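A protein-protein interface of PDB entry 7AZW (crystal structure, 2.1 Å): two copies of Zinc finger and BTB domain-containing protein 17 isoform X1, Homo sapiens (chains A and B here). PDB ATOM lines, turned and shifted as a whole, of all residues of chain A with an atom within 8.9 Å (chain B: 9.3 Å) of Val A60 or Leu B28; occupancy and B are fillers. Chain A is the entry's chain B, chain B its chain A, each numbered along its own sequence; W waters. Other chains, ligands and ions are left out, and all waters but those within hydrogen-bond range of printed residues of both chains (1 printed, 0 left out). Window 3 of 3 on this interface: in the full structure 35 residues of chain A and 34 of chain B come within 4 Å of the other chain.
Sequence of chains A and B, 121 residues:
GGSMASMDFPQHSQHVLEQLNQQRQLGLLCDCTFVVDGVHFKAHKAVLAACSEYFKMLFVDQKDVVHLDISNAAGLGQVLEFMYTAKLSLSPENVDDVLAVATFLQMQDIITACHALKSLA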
ATOM      1  N   LYS A  45     -18.437  31.074  10.742  1.00  0.00           N
ATOM      2  CA  LYS A  45     -19.081  30.080   9.887  1.00  0.00           C
ATOM      3  C   LYS A  45     -18.077  29.058   9.369  1.00  0.00           C
ATOM      4  O   LYS A  45     -18.387  27.863   9.274  1.00  0.00           O
ATOM      5  CB  LYS A  45     -19.779  30.767   8.714  1.00  0.00           C
ATOM      6  CG  LYS A  45     -21.082  31.460   9.059  1.00  0.00           C
ATOM      7  CD  LYS A  45     -21.608  32.225   7.854  1.00  0.00           C
ATOM      8  CE  LYS A  45     -23.055  32.636   8.044  1.00  0.00           C
ATOM      9  NZ  LYS A  45     -23.550  33.448   6.897  1.00  0.00           N
ATOM     10  N   ALA A  46     -16.869  29.509   9.025  1.00  0.00           N
ATOM     11  CA  ALA A  46     -15.865  28.604   8.473  1.00  0.00           C
ATOM     12  C   ALA A  46     -15.404  27.584   9.508  1.00  0.00           C
ATOM     13  O   ALA A  46     -15.175  26.416   9.175  1.00  0.00           O
ATOM     14  CB  ALA A  46     -14.677  29.402   7.937  1.00  0.00           C
ATOM     15  N   ALA A  49     -18.288  25.004   9.929  1.00  0.00           N
ATOM     16  CA  ALA A  49     -18.336  24.064   8.815  1.00  0.00           C
ATOM     17  C   ALA A  49     -17.172  23.085   8.856  1.00  0.00           C
ATOM     18  O   ALA A  49     -17.304  21.948   8.391  1.00  0.00           O
ATOM     19  CB  ALA A  49     -18.350  24.825   7.490  1.00  0.00           C
ATOM     20  N   ALA A  50     -16.035  23.498   9.413  1.00  0.00           N
ATOM     21  CA  ALA A  50     -14.875  22.623   9.513  1.00  0.00           C
ATOM     22  C   ALA A  50     -15.024  21.546  10.580  1.00  0.00           C
ATOM     23  O   ALA A  50     -14.209  20.618  10.612  1.00  0.00           O
ATOM     24  CB  ALA A  50     -13.620  23.453   9.792  1.00  0.00           C
ATOM     25  N   SER A  52     -18.574  20.551  11.937  1.00  0.00           N
ATOM     26  CA  SER A  52     -19.909  19.968  11.945  1.00  0.00           C
ATOM     27  C   SER A  52     -20.423  19.852  10.519  1.00  0.00           C
ATOM     28  O   SER A  52     -20.405  20.832   9.766  1.00  0.00           O
ATOM     29  CB  SER A  52     -20.879  20.804  12.788  1.00  0.00           C
ATOM     30  OG  SER A  52     -22.188  20.266  12.721  1.00  0.00           O
ATOM     31  N   GLU A  53     -20.886  18.653  10.156  1.00  0.00           N
ATOM     32  CA  GLU A  53     -21.455  18.452   8.827  1.00  0.00           C
ATOM     33  C   GLU A  53     -22.768  19.205   8.657  1.00  0.00           C
ATOM     34  O   GLU A  53     -23.085  19.653   7.548  1.00  0.00           O
ATOM     35  CB  GLU A  53     -21.655  16.958   8.567  1.00  0.00           C
ATOM     36  CG  GLU A  53     -22.308  16.619   7.231  1.00  0.00           C
ATOM     37  CD  GLU A  53     -21.385  16.831   6.042  1.00  0.00           C
ATOM     38  OE1 GLU A  53     -20.196  17.160   6.246  1.00  0.00           O
ATOM     39  OE2 GLU A  53     -21.852  16.663   4.895  1.00  0.00           O
ATOM     40  N   TYR A  54     -23.546  19.352   9.735  1.00  0.00           N
ATOM     41  CA  TYR A  54     -24.783  20.124   9.654  1.00  0.00           C
ATOM     42  C   TYR A  54     -24.500  21.564   9.246  1.00  0.00           C
ATOM     43  O   TYR A  54     -25.153  22.108   8.348  1.00  0.00           O
ATOM     44  CB  TYR A  54     -25.524  20.084  10.992  1.00  0.00           C
ATOM     45  CG  TYR A  54     -26.648  21.096  11.072  1.00  0.00           C
ATOM     46  CD1 TYR A  54     -27.888  20.825  10.509  1.00  0.00           C
ATOM     47  CD2 TYR A  54     -26.463  22.328  11.690  1.00  0.00           C
ATOM     48  CE1 TYR A  54     -28.914  21.747  10.567  1.00  0.00           C
ATOM     49  CE2 TYR A  54     -27.484  23.256  11.752  1.00  0.00           C
ATOM     50  CZ  TYR A  54     -28.707  22.961  11.189  1.00  0.00           C
ATOM     51  OH  TYR A  54     -29.728  23.882  11.248  1.00  0.00           O
ATOM     52  N   PHE A  55     -23.530  22.201   9.905  1.00  0.00           N
ATOM     53  CA  PHE A  55     -23.191  23.580   9.570  1.00  0.00           C
ATOM     54  C   PHE A  55     -22.544  23.670   8.195  1.00  0.00           C
ATOM     55  O   PHE A  55     -22.771  24.638   7.459  1.00  0.00           O
ATOM     56  CB  PHE A  55     -22.268  24.165  10.639  1.00  0.00           C
ATOM     57  CG  PHE A  55     -22.990  24.657  11.859  1.00  0.00           C
ATOM     58  CD1 PHE A  55     -24.074  25.513  11.742  1.00  0.00           C
ATOM     59  CD2 PHE A  55     -22.586  24.265  13.123  1.00  0.00           C
ATOM     60  CE1 PHE A  55     -24.738  25.969  12.863  1.00  0.00           C
ATOM     61  CE2 PHE A  55     -23.248  24.719  14.247  1.00  0.00           C
ATOM     62  CZ  PHE A  55     -24.324  25.571  14.117  1.00  0.00           C
ATOM     63  N   LYS A  56     -21.734  22.673   7.833  1.00  0.00           N
ATOM     64  CA  LYS A  56     -21.116  22.657   6.511  1.00  0.00           C
ATOM     65  C   LYS A  56     -22.172  22.645   5.413  1.00  0.00           C
ATOM     66  O   LYS A  56     -22.122  23.450   4.476  1.00  0.00           O
ATOM     67  CB  LYS A  56     -20.187  21.449   6.383  1.00  0.00           C
ATOM     68  CG  LYS A  56     -19.439  21.376   5.061  1.00  0.00           C
ATOM     69  CD  LYS A  56     -18.554  20.144   4.998  1.00  0.00           C
ATOM     70  CE  LYS A  56     -17.719  20.127   3.729  1.00  0.00           C
ATOM     71  NZ  LYS A  56     -16.821  18.941   3.669  1.00  0.00           N
ATOM     72  N   MET A  57     -23.147  21.739   5.519  1.00  0.00           N
ATOM     73  CA  MET A  57     -24.214  21.686   4.526  1.00  0.00           C
ATOM     74  C   MET A  57     -25.089  22.931   4.568  1.00  0.00           C
ATOM     75  O   MET A  57     -25.639  23.336   3.539  1.00  0.00           O
ATOM     76  CB  MET A  57     -25.065  20.434   4.738  1.00  0.00           C
ATOM     77  CG  MET A  57     -24.362  19.139   4.375  1.00  0.00           C
ATOM     78  SD  MET A  57     -23.983  19.045   2.616  1.00  0.00           S
ATOM     79  CE  MET A  57     -25.613  19.276   1.913  1.00  0.00           C
ATOM     80  N   LEU A  58     -25.225  23.554   5.741  1.00  0.00           N
ATOM     81  CA  LEU A  58     -26.072  24.735   5.861  1.00  0.00           C
ATOM     82  C   LEU A  58     -25.389  25.981   5.307  1.00  0.00           C
ATOM     83  O   LEU A  58     -26.018  26.772   4.596  1.00  0.00           O
ATOM     84  CB  LEU A  58     -26.466  24.951   7.322  1.00  0.00           C
ATOM     85  CG  LEU A  58     -27.461  26.079   7.602  1.00  0.00           C
ATOM     86  CD1 LEU A  58     -28.849  25.707   7.104  1.00  0.00           C
ATOM     87  CD2 LEU A  58     -27.486  26.411   9.086  1.00  0.00           C
ATOM     88  N   PHE A  59     -24.104  26.168   5.615  1.00  0.00           N
ATOM     89  CA  PHE A  59     -23.412  27.388   5.211  1.00  0.00           C
ATOM     90  C   PHE A  59     -22.944  27.338   3.761  1.00  0.00           C
ATOM     91  O   PHE A  59     -22.898  28.381   3.098  1.00  0.00           O
ATOM     92  CB  PHE A  59     -22.229  27.651   6.143  1.00  0.00           C
ATOM     93  CG  PHE A  59     -22.632  28.060   7.531  1.00  0.00           C
ATOM     94  CD1 PHE A  59     -23.754  28.847   7.738  1.00  0.00           C
ATOM     95  CD2 PHE A  59     -21.893  27.655   8.630  1.00  0.00           C
ATOM     96  CE1 PHE A  59     -24.127  29.224   9.013  1.00  0.00           C
ATOM     97  CE2 PHE A  59     -22.262  28.030   9.907  1.00  0.00           C
ATOM     98  CZ  PHE A  59     -23.382  28.815  10.100  1.00  0.00           C
ATOM     99  N   VAL A  60     -22.595  26.154   3.252  1.00  0.00           N
ATOM    100  CA  VAL A  60     -22.217  26.044   1.846  1.00  0.00           C
ATOM    101  C   VAL A  60     -23.430  26.272   0.951  1.00  0.00           C
ATOM    102  O   VAL A  60     -23.306  26.827  -0.149  1.00  0.00           O
ATOM    103  CB  VAL A  60     -21.545  24.683   1.577  1.00  0.00           C
ATOM    104  CG1 VAL A  60     -21.399  24.428   0.084  1.00  0.00           C
ATOM    105  CG2 VAL A  60     -20.183  24.631   2.254  1.00  0.00           C
ATOM    106  N   ASP A  61     -24.620  25.879   1.409  1.00  0.00           N
ATOM    107  CA  ASP A  61     -25.859  26.203   0.710  1.00  0.00           C
ATOM    108  C   ASP A  61     -26.189  27.691   0.754  1.00  0.00           C
ATOM    109  O   ASP A  61     -27.255  28.085   0.267  1.00  0.00           O
ATOM    110  CB  ASP A  61     -27.016  25.392   1.304  1.00  0.00           C
ATOM    111  CG  ASP A  61     -28.186  25.256   0.349  1.00  0.00           C
ATOM    112  OD1 ASP A  61     -27.981  25.429  -0.871  1.00  0.00           O
ATOM    113  OD2 ASP A  61     -29.310  24.980   0.820  1.00  0.00           O
ATOM    114  N   GLN A  62     -25.304  28.517   1.321  1.00  0.00           N
ATOM    115  CA  GLN A  62     -25.524  29.956   1.466  1.00  0.00           C
ATOM    116  C   GLN A  62     -26.784  30.240   2.278  1.00  0.00           C
ATOM    117  O   GLN A  62     -27.539  31.169   1.988  1.00  0.00           O
ATOM    118  CB  GLN A  62     -25.577  30.654   0.104  1.00  0.00           C
ATOM    119  CG  GLN A  62     -24.260  30.628  -0.650  1.00  0.00           C
ATOM    120  CD  GLN A  62     -23.137  31.294   0.118  1.00  0.00           C
ATOM    121  OE1 GLN A  62     -23.184  32.494   0.393  1.00  0.00           O
ATOM    122  NE2 GLN A  62     -22.119  30.518   0.473  1.00  0.00           N
ATOM    123  N   LYS A  63     -27.013  29.428   3.305  1.00  0.00           N
ATOM    124  CA  LYS A  63     -28.126  29.617   4.219  1.00  0.00           C
ATOM    125  C   LYS A  63     -27.613  30.088   5.571  1.00  0.00           C
ATOM    126  O   LYS A  63     -26.502  29.747   5.991  1.00  0.00           O
ATOM    127  CB  LYS A  63     -28.934  28.327   4.391  1.00  0.00           C
ATOM    128  CG  LYS A  63     -29.648  27.866   3.130  1.00  0.00           C
ATOM    129  CD  LYS A  63     -30.396  29.009   2.454  1.00  0.00           C
ATOM    130  CE  LYS A  63     -31.539  29.525   3.317  1.00  0.00           C
ATOM    131  NZ  LYS A  63     -32.067  30.823   2.814  1.00  0.00           N
ATOM    132  N   ASP A  64     -28.433  30.882   6.244  1.00  0.00           N
ATOM    133  CA  ASP A  64     -28.111  31.416   7.556  1.00  0.00           C
ATOM    134  C   ASP A  64     -28.959  30.727   8.617  1.00  0.00           C
ATOM    135  O   ASP A  64     -29.914  30.004   8.319  1.00  0.00           O
ATOM    136  CB  ASP A  64     -28.323  32.933   7.594  1.00  0.00           C
ATOM    137  CG  ASP A  64     -27.086  33.706   7.165  1.00  0.00           C
ATOM    138  OD1 ASP A  64     -26.067  33.666   7.886  1.00  0.00           O
ATOM    139  OD2 ASP A  64     -27.130  34.346   6.093  1.00  0.00           O
ATOM    140  N   GLN B  19      -9.428  21.246   6.996  1.00  0.00           N
ATOM    141  CA  GLN B  19     -10.759  21.529   6.470  1.00  0.00           C
ATOM    142  C   GLN B  19     -10.859  22.964   5.969  1.00  0.00           C
ATOM    143  O   GLN B  19     -11.506  23.228   4.950  1.00  0.00           O
ATOM    144  CB  GLN B  19     -11.815  21.259   7.541  1.00  0.00           C
ATOM    145  CG  GLN B  19     -12.037  19.785   7.836  1.00  0.00           C
ATOM    146  CD  GLN B  19     -12.747  19.070   6.705  1.00  0.00           C
ATOM    147  OE1 GLN B  19     -13.860  19.433   6.328  1.00  0.00           O
ATOM    148  NE2 GLN B  19     -12.103  18.045   6.157  1.00  0.00           N
ATOM    149  N   LEU B  20     -10.220  23.905   6.672  1.00  0.00           N
ATOM    150  CA  LEU B  20     -10.215  25.289   6.214  1.00  0.00           C
ATOM    151  C   LEU B  20      -9.438  25.435   4.912  1.00  0.00           C
ATOM    152  O   LEU B  20      -9.814  26.229   4.043  1.00  0.00           O
ATOM    153  CB  LEU B  20      -9.631  26.199   7.295  1.00  0.00           C
ATOM    154  CG  LEU B  20     -10.481  26.378   8.555  1.00  0.00           C
ATOM    155  CD1 LEU B  20      -9.697  27.103   9.637  1.00  0.00           C
ATOM    156  CD2 LEU B  20     -11.766  27.123   8.230  1.00  0.00           C
ATOM    157  N   ASN B  21      -8.350  24.676   4.760  1.00  0.00           N
ATOM    158  CA  ASN B  21      -7.616  24.686   3.500  1.00  0.00           C
ATOM    159  C   ASN B  21      -8.429  24.054   2.378  1.00  0.00           C
ATOM    160  O   ASN B  21      -8.292  24.451   1.216  1.00  0.00           O
ATOM    161  CB  ASN B  21      -6.278  23.965   3.660  1.00  0.00           C
ATOM    162  CG  ASN B  21      -5.331  24.232   2.505  1.00  0.00           C
ATOM    163  OD1 ASN B  21      -5.253  25.350   1.996  1.00  0.00           O
ATOM    164  ND2 ASN B  21      -4.608  23.201   2.084  1.00  0.00           N
ATOM    165  N   GLN B  22      -9.276  23.074   2.704  1.00  0.00           N
ATOM    166  CA  GLN B  22     -10.147  22.488   1.691  1.00  0.00           C
ATOM    167  C   GLN B  22     -11.233  23.468   1.268  1.00  0.00           C
ATOM    168  O   GLN B  22     -11.584  23.539   0.084  1.00  0.00           O
ATOM    169  CB  GLN B  22     -10.764  21.190   2.214  1.00  0.00           C
ATOM    170  CG  GLN B  22     -11.587  20.439   1.181  1.00  0.00           C
ATOM    171  CD  GLN B  22     -12.647  19.557   1.809  1.00  0.00           C
ATOM    172  OE1 GLN B  22     -13.844  19.782   1.631  1.00  0.00           O
ATOM    173  NE2 GLN B  22     -12.211  18.541   2.547  1.00  0.00           N
ATOM    174  N   GLN B  23     -11.781  24.227   2.222  1.00  0.00           N
ATOM    175  CA  GLN B  23     -12.722  25.287   1.874  1.00  0.00           C
ATOM    176  C   GLN B  23     -12.078  26.306   0.944  1.00  0.00           C
ATOM    177  O   GLN B  23     -12.714  26.784  -0.003  1.00  0.00           O
ATOM    178  CB  GLN B  23     -13.233  25.981   3.138  1.00  0.00           C
ATOM    179  CG  GLN B  23     -13.987  25.089   4.105  1.00  0.00           C
ATOM    180  CD  GLN B  23     -14.326  25.807   5.397  1.00  0.00           C
ATOM    181  OE1 GLN B  23     -14.171  27.025   5.503  1.00  0.00           O
ATOM    182  NE2 GLN B  23     -14.792  25.056   6.389  1.00  0.00           N
ATOM    183  N   ARG B  24     -10.815  26.649   1.200  1.00  0.00           N
ATOM    184  CA  ARG B  24     -10.128  27.644   0.383  1.00  0.00           C
ATOM    185  C   ARG B  24      -9.936  27.148  -1.045  1.00  0.00           C
ATOM    186  O   ARG B  24     -10.196  27.879  -2.008  1.00  0.00           O
ATOM    187  CB  ARG B  24      -8.781  27.997   1.013  1.00  0.00           C
ATOM    188  CG  ARG B  24      -7.939  28.933   0.166  1.00  0.00           C
ATOM    189  CD  ARG B  24      -6.622  29.271   0.846  1.00  0.00           C
ATOM    190  NE  ARG B  24      -5.675  28.161   0.806  1.00  0.00           N
ATOM    191  CZ  ARG B  24      -4.732  28.015  -0.121  1.00  0.00           C
ATOM    192  NH1 ARG B  24      -4.612  28.910  -1.092  1.00  0.00           N
ATOM    193  NH2 ARG B  24      -3.911  26.975  -0.080  1.00  0.00           N
ATOM    194  N   GLN B  25      -9.477  25.903  -1.200  1.00  0.00           N
ATOM    195  CA  GLN B  25      -9.221  25.366  -2.533  1.00  0.00           C
ATOM    196  C   GLN B  25     -10.486  25.329  -3.381  1.00  0.00           C
ATOM    197  O   GLN B  25     -10.414  25.472  -4.606  1.00  0.00           O
ATOM    198  CB  GLN B  25      -8.608  23.970  -2.426  1.00  0.00           C
ATOM    199  CG  GLN B  25      -7.196  23.956  -1.859  1.00  0.00           C
ATOM    200  CD  GLN B  25      -6.698  22.556  -1.562  1.00  0.00           C
ATOM    201  OE1 GLN B  25      -7.338  21.797  -0.833  1.00  0.00           O
ATOM    202  NE2 GLN B  25      -5.548  22.204  -2.126  1.00  0.00           N
ATOM    203  N   LEU B  26     -11.646  25.144  -2.753  1.00  0.00           N
ATOM    204  CA  LEU B  26     -12.916  25.168  -3.466  1.00  0.00           C
ATOM    205  C   LEU B  26     -13.567  26.546  -3.475  1.00  0.00           C
ATOM    206  O   LEU B  26     -14.590  26.725  -4.143  1.00  0.00           O
ATOM    207  CB  LEU B  26     -13.888  24.153  -2.854  1.00  0.00           C
ATOM    208  CG  LEU B  26     -13.400  22.706  -2.751  1.00  0.00           C
ATOM    209  CD1 LEU B  26     -14.529  21.790  -2.304  1.00  0.00           C
ATOM    210  CD2 LEU B  26     -12.814  22.236  -4.074  1.00  0.00           C
ATOM    211  N   GLY B  27     -13.004  27.516  -2.757  1.00  0.00           N
ATOM    212  CA  GLY B  27     -13.577  28.847  -2.725  1.00  0.00           C
ATOM    213  C   GLY B  27     -14.820  28.985  -1.880  1.00  0.00           C
ATOM    214  O   GLY B  27     -15.557  29.963  -2.036  1.00  0.00           O
ATOM    215  N   LEU B  28     -15.076  28.039  -0.981  1.00  0.00           N
ATOM    216  CA  LEU B  28     -16.267  28.069  -0.146  1.00  0.00           C
ATOM    217  C   LEU B  28     -15.990  28.831   1.143  1.00  0.00           C
ATOM    218  O   LEU B  28     -14.963  28.610   1.795  1.00  0.00           O
ATOM    219  CB  LEU B  28     -16.743  26.651   0.173  1.00  0.00           C
ATOM    220  CG  LEU B  28     -16.846  25.674  -1.001  1.00  0.00           C
ATOM    221  CD1 LEU B  28     -16.691  24.234  -0.526  1.00  0.00           C
ATOM    222  CD2 LEU B  28     -18.158  25.858  -1.747  1.00  0.00           C
ATOM    223  N   LEU B  29     -16.911  29.728   1.498  1.00  0.00           N
ATOM    224  CA  LEU B  29     -16.891  30.481   2.751  1.00  0.00           C
ATOM    225  C   LEU B  29     -15.686  31.410   2.864  1.00  0.00           C
ATOM    226  O   LEU B  29     -15.339  31.850   3.965  1.00  0.00           O
ATOM    227  CB  LEU B  29     -16.954  29.544   3.962  1.00  0.00           C
ATOM    228  CG  LEU B  29     -18.097  28.527   3.949  1.00  0.00           C
ATOM    229  CD1 LEU B  29     -18.076  27.676   5.208  1.00  0.00           C
ATOM    230  CD2 LEU B  29     -19.444  29.221   3.792  1.00  0.00           C
ATOM    231  N   CYS B  30     -15.039  31.725   1.746  1.00  0.00           N
ATOM    232  CA  CYS B  30     -13.962  32.704   1.756  1.00  0.00           C
ATOM    233  C   CYS B  30     -14.536  34.104   1.597  1.00  0.00           C
ATOM    234  O   CYS B  30     -15.448  34.328   0.798  1.00  0.00           O
ATOM    235  CB  CYS B  30     -12.959  32.418   0.638  1.00  0.00           C
ATOM    236  SG  CYS B  30     -12.119  30.828   0.768  1.00  0.00           S
ATOM    237  N   ASP B  31     -13.984  35.053   2.358  1.00  0.00           N
ATOM    238  CA  ASP B  31     -14.512  36.411   2.389  1.00  0.00           C
ATOM    239  C   ASP B  31     -13.452  37.483   2.156  1.00  0.00           C
ATOM    240  O   ASP B  31     -13.734  38.668   2.372  1.00  0.00           O
ATOM    241  CB  ASP B  31     -15.224  36.668   3.722  1.00  0.00           C
ATOM    242  CG  ASP B  31     -14.364  36.310   4.924  1.00  0.00           C
ATOM    243  OD1 ASP B  31     -13.232  35.821   4.729  1.00  0.00           O
ATOM    244  OD2 ASP B  31     -14.822  36.518   6.067  1.00  0.00           O
ATOM    245  N   CYS B  32     -12.247  37.112   1.726  1.00  0.00           N
ATOM    246  CA  CYS B  32     -11.206  38.086   1.427  1.00  0.00           C
ATOM    247  C   CYS B  32     -10.449  37.637   0.184  1.00  0.00           C
ATOM    248  O   CYS B  32     -10.712  36.569  -0.376  1.00  0.00           O
ATOM    249  CB  CYS B  32     -10.250  38.269   2.611  1.00  0.00           C
ATOM    250  SG  CYS B  32      -9.220  36.827   2.991  1.00  0.00           S
ATOM    251  N   LYS B  42      -8.288  33.469  -2.988  1.00  0.00           N
ATOM    252  CA  LYS B  42      -9.314  33.530  -1.957  1.00  0.00           C
ATOM    253  C   LYS B  42      -8.793  32.963  -0.640  1.00  0.00           C
ATOM    254  O   LYS B  42      -7.934  32.078  -0.616  1.00  0.00           O
ATOM    255  CB  LYS B  42     -10.560  32.764  -2.399  1.00  0.00           C
ATOM    256  CG  LYS B  42     -11.233  33.330  -3.640  1.00  0.00           C
ATOM    257  CD  LYS B  42     -12.347  32.415  -4.126  1.00  0.00           C
ATOM    258  CE  LYS B  42     -12.965  32.931  -5.417  1.00  0.00           C
ATOM    259  NZ  LYS B  42     -13.493  31.827  -6.267  1.00  0.00           N
ATOM    260  N   ALA B  43      -9.329  33.479   0.463  1.00  0.00           N
ATOM    261  CA  ALA B  43      -8.923  33.051   1.796  1.00  0.00           C
ATOM    262  C   ALA B  43      -9.973  33.517   2.798  1.00  0.00           C
ATOM    263  O   ALA B  43     -10.954  34.175   2.441  1.00  0.00           O
ATOM    264  CB  ALA B  43      -7.535  33.588   2.151  1.00  0.00           C
ATOM    265  N   HIS B  44      -9.756  33.169   4.064  1.00  0.00           N
ATOM    266  CA  HIS B  44     -10.637  33.566   5.156  1.00  0.00           C
ATOM    267  C   HIS B  44      -9.999  34.709   5.934  1.00  0.00           C
ATOM    268  O   HIS B  44      -8.826  34.626   6.310  1.00  0.00           O
ATOM    269  CB  HIS B  44     -10.918  32.392   6.095  1.00  0.00           C
ATOM    270  CG  HIS B  44     -11.437  31.169   5.405  1.00  0.00           C
ATOM    271  ND1 HIS B  44     -10.613  30.159   4.960  1.00  0.00           N
ATOM    272  CD2 HIS B  44     -12.700  30.791   5.095  1.00  0.00           C
ATOM    273  CE1 HIS B  44     -11.345  29.212   4.400  1.00  0.00           C
ATOM    274  NE2 HIS B  44     -12.613  29.571   4.468  1.00  0.00           N
ATOM    275  N   TYR B  84      -2.161  28.132   5.794  1.00  0.00           N
ATOM    276  CA  TYR B  84      -3.148  27.069   5.668  1.00  0.00           C
ATOM    277  C   TYR B  84      -2.554  25.671   5.768  1.00  0.00           C
ATOM    278  O   TYR B  84      -3.282  24.734   6.108  1.00  0.00           O
ATOM    279  CB  TYR B  84      -3.903  27.202   4.339  1.00  0.00           C
ATOM    280  CG  TYR B  84      -5.001  28.241   4.369  1.00  0.00           C
ATOM    281  CD1 TYR B  84      -6.293  27.899   4.746  1.00  0.00           C
ATOM    282  CD2 TYR B  84      -4.748  29.562   4.022  1.00  0.00           C
ATOM    283  CE1 TYR B  84      -7.302  28.843   4.779  1.00  0.00           C
ATOM    284  CE2 TYR B  84      -5.754  30.515   4.052  1.00  0.00           C
ATOM    285  CZ  TYR B  84      -7.029  30.148   4.431  1.00  0.00           C
ATOM    286  OH  TYR B  84      -8.036  31.086   4.463  1.00  0.00           O
HETATM  287  O   HOH W   1     -15.551  22.494   6.067  1.00  0.00           O
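No position is printed for both chains.
The backbone carbonyl oxygen (O) of Gln B23 sits at hydrogen-bond distance from the backbone NH (N) of Leu B28 (2.8 Å).
OE1 of Gln B23 is in hydrogen-bond range of NE2 of His B44 (3.2 Å).
The side-chain sulfur (SG) of Cys B30 is in hydrogen-bond range of the backbone carbonyl oxygen (O) of Leu B28, 3.8 Å away.
N of His B44 sits at hydrogen-bond distance from OH of Tyr B84, at 2.7 Å.
O of Phe A59 sits close to NE2 of Gln A62 (3.5 Å).
Water W1 lies within hydrogen-bond range of NE2 of Gln B23 (2.7 Å) and O of Ala A49 (3.0 Å).
Among the printed residues, merely in contact across the chains: Ala A46 with Leu B20, Ala A50 with Gln B23, Phe A59 with Leu B29, Ala A50 with Gln B19, Ala A49 with Leu B29, Lys A56 with Gln B22, Ala A46 with His B44, Ala A49 with Gln B23 and Val A60 with Leu B28.
Of the printed residues of chain B, Val A60 touches Leu B28 (3.99 Å).
Of the printed residues of chain A, Leu B28 touches Val A60.
Of chain A, only Ala A49 and Phe A59 come within 4 Å of Leu B29.
Of the printed residues of chain B, Ala A49 touches Gln B23 (3.7 Å) and Leu B29 (3.7 Å).
Printed residues of chain A within 4 Å of His B44: Ala A46.
Printed residues of chain A within 4 Å of Leu B20: Ala A46.
Asp A61 touches none of the printed residues of chain B.
Gln A62 touches none of the printed residues of chain B.
The nearest printed residue of chain A that does not touch Leu B28 is Lys A56 (6.0 Å).
The backbone carbonyl oxygen of Ala A46 lies within hydrogen-bond range of the side-chain amide nitrogen of Gln B23 (3.1 Å).
Of the 17 printed residues of chain A, 6 touch a printed residue of chain B.
Hydrophobic or aromatic side chains of chain A within 4 Å of the printed part of chain B: Ala A46, Ala A49, Ala A50, Phe A59 and Val A60.
Hydrophobic or aromatic side chains of chain B within 4 Å of the printed part of chain A: Leu B20, Leu B28, Leu B29 and His B44.
Among the printed residues, 10 pairs touch across the chains.
Among the printed residues, no Asp or Glu carboxylate lies within 4 Å of a Lys or Arg side-chain nitrogen of the other chain.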
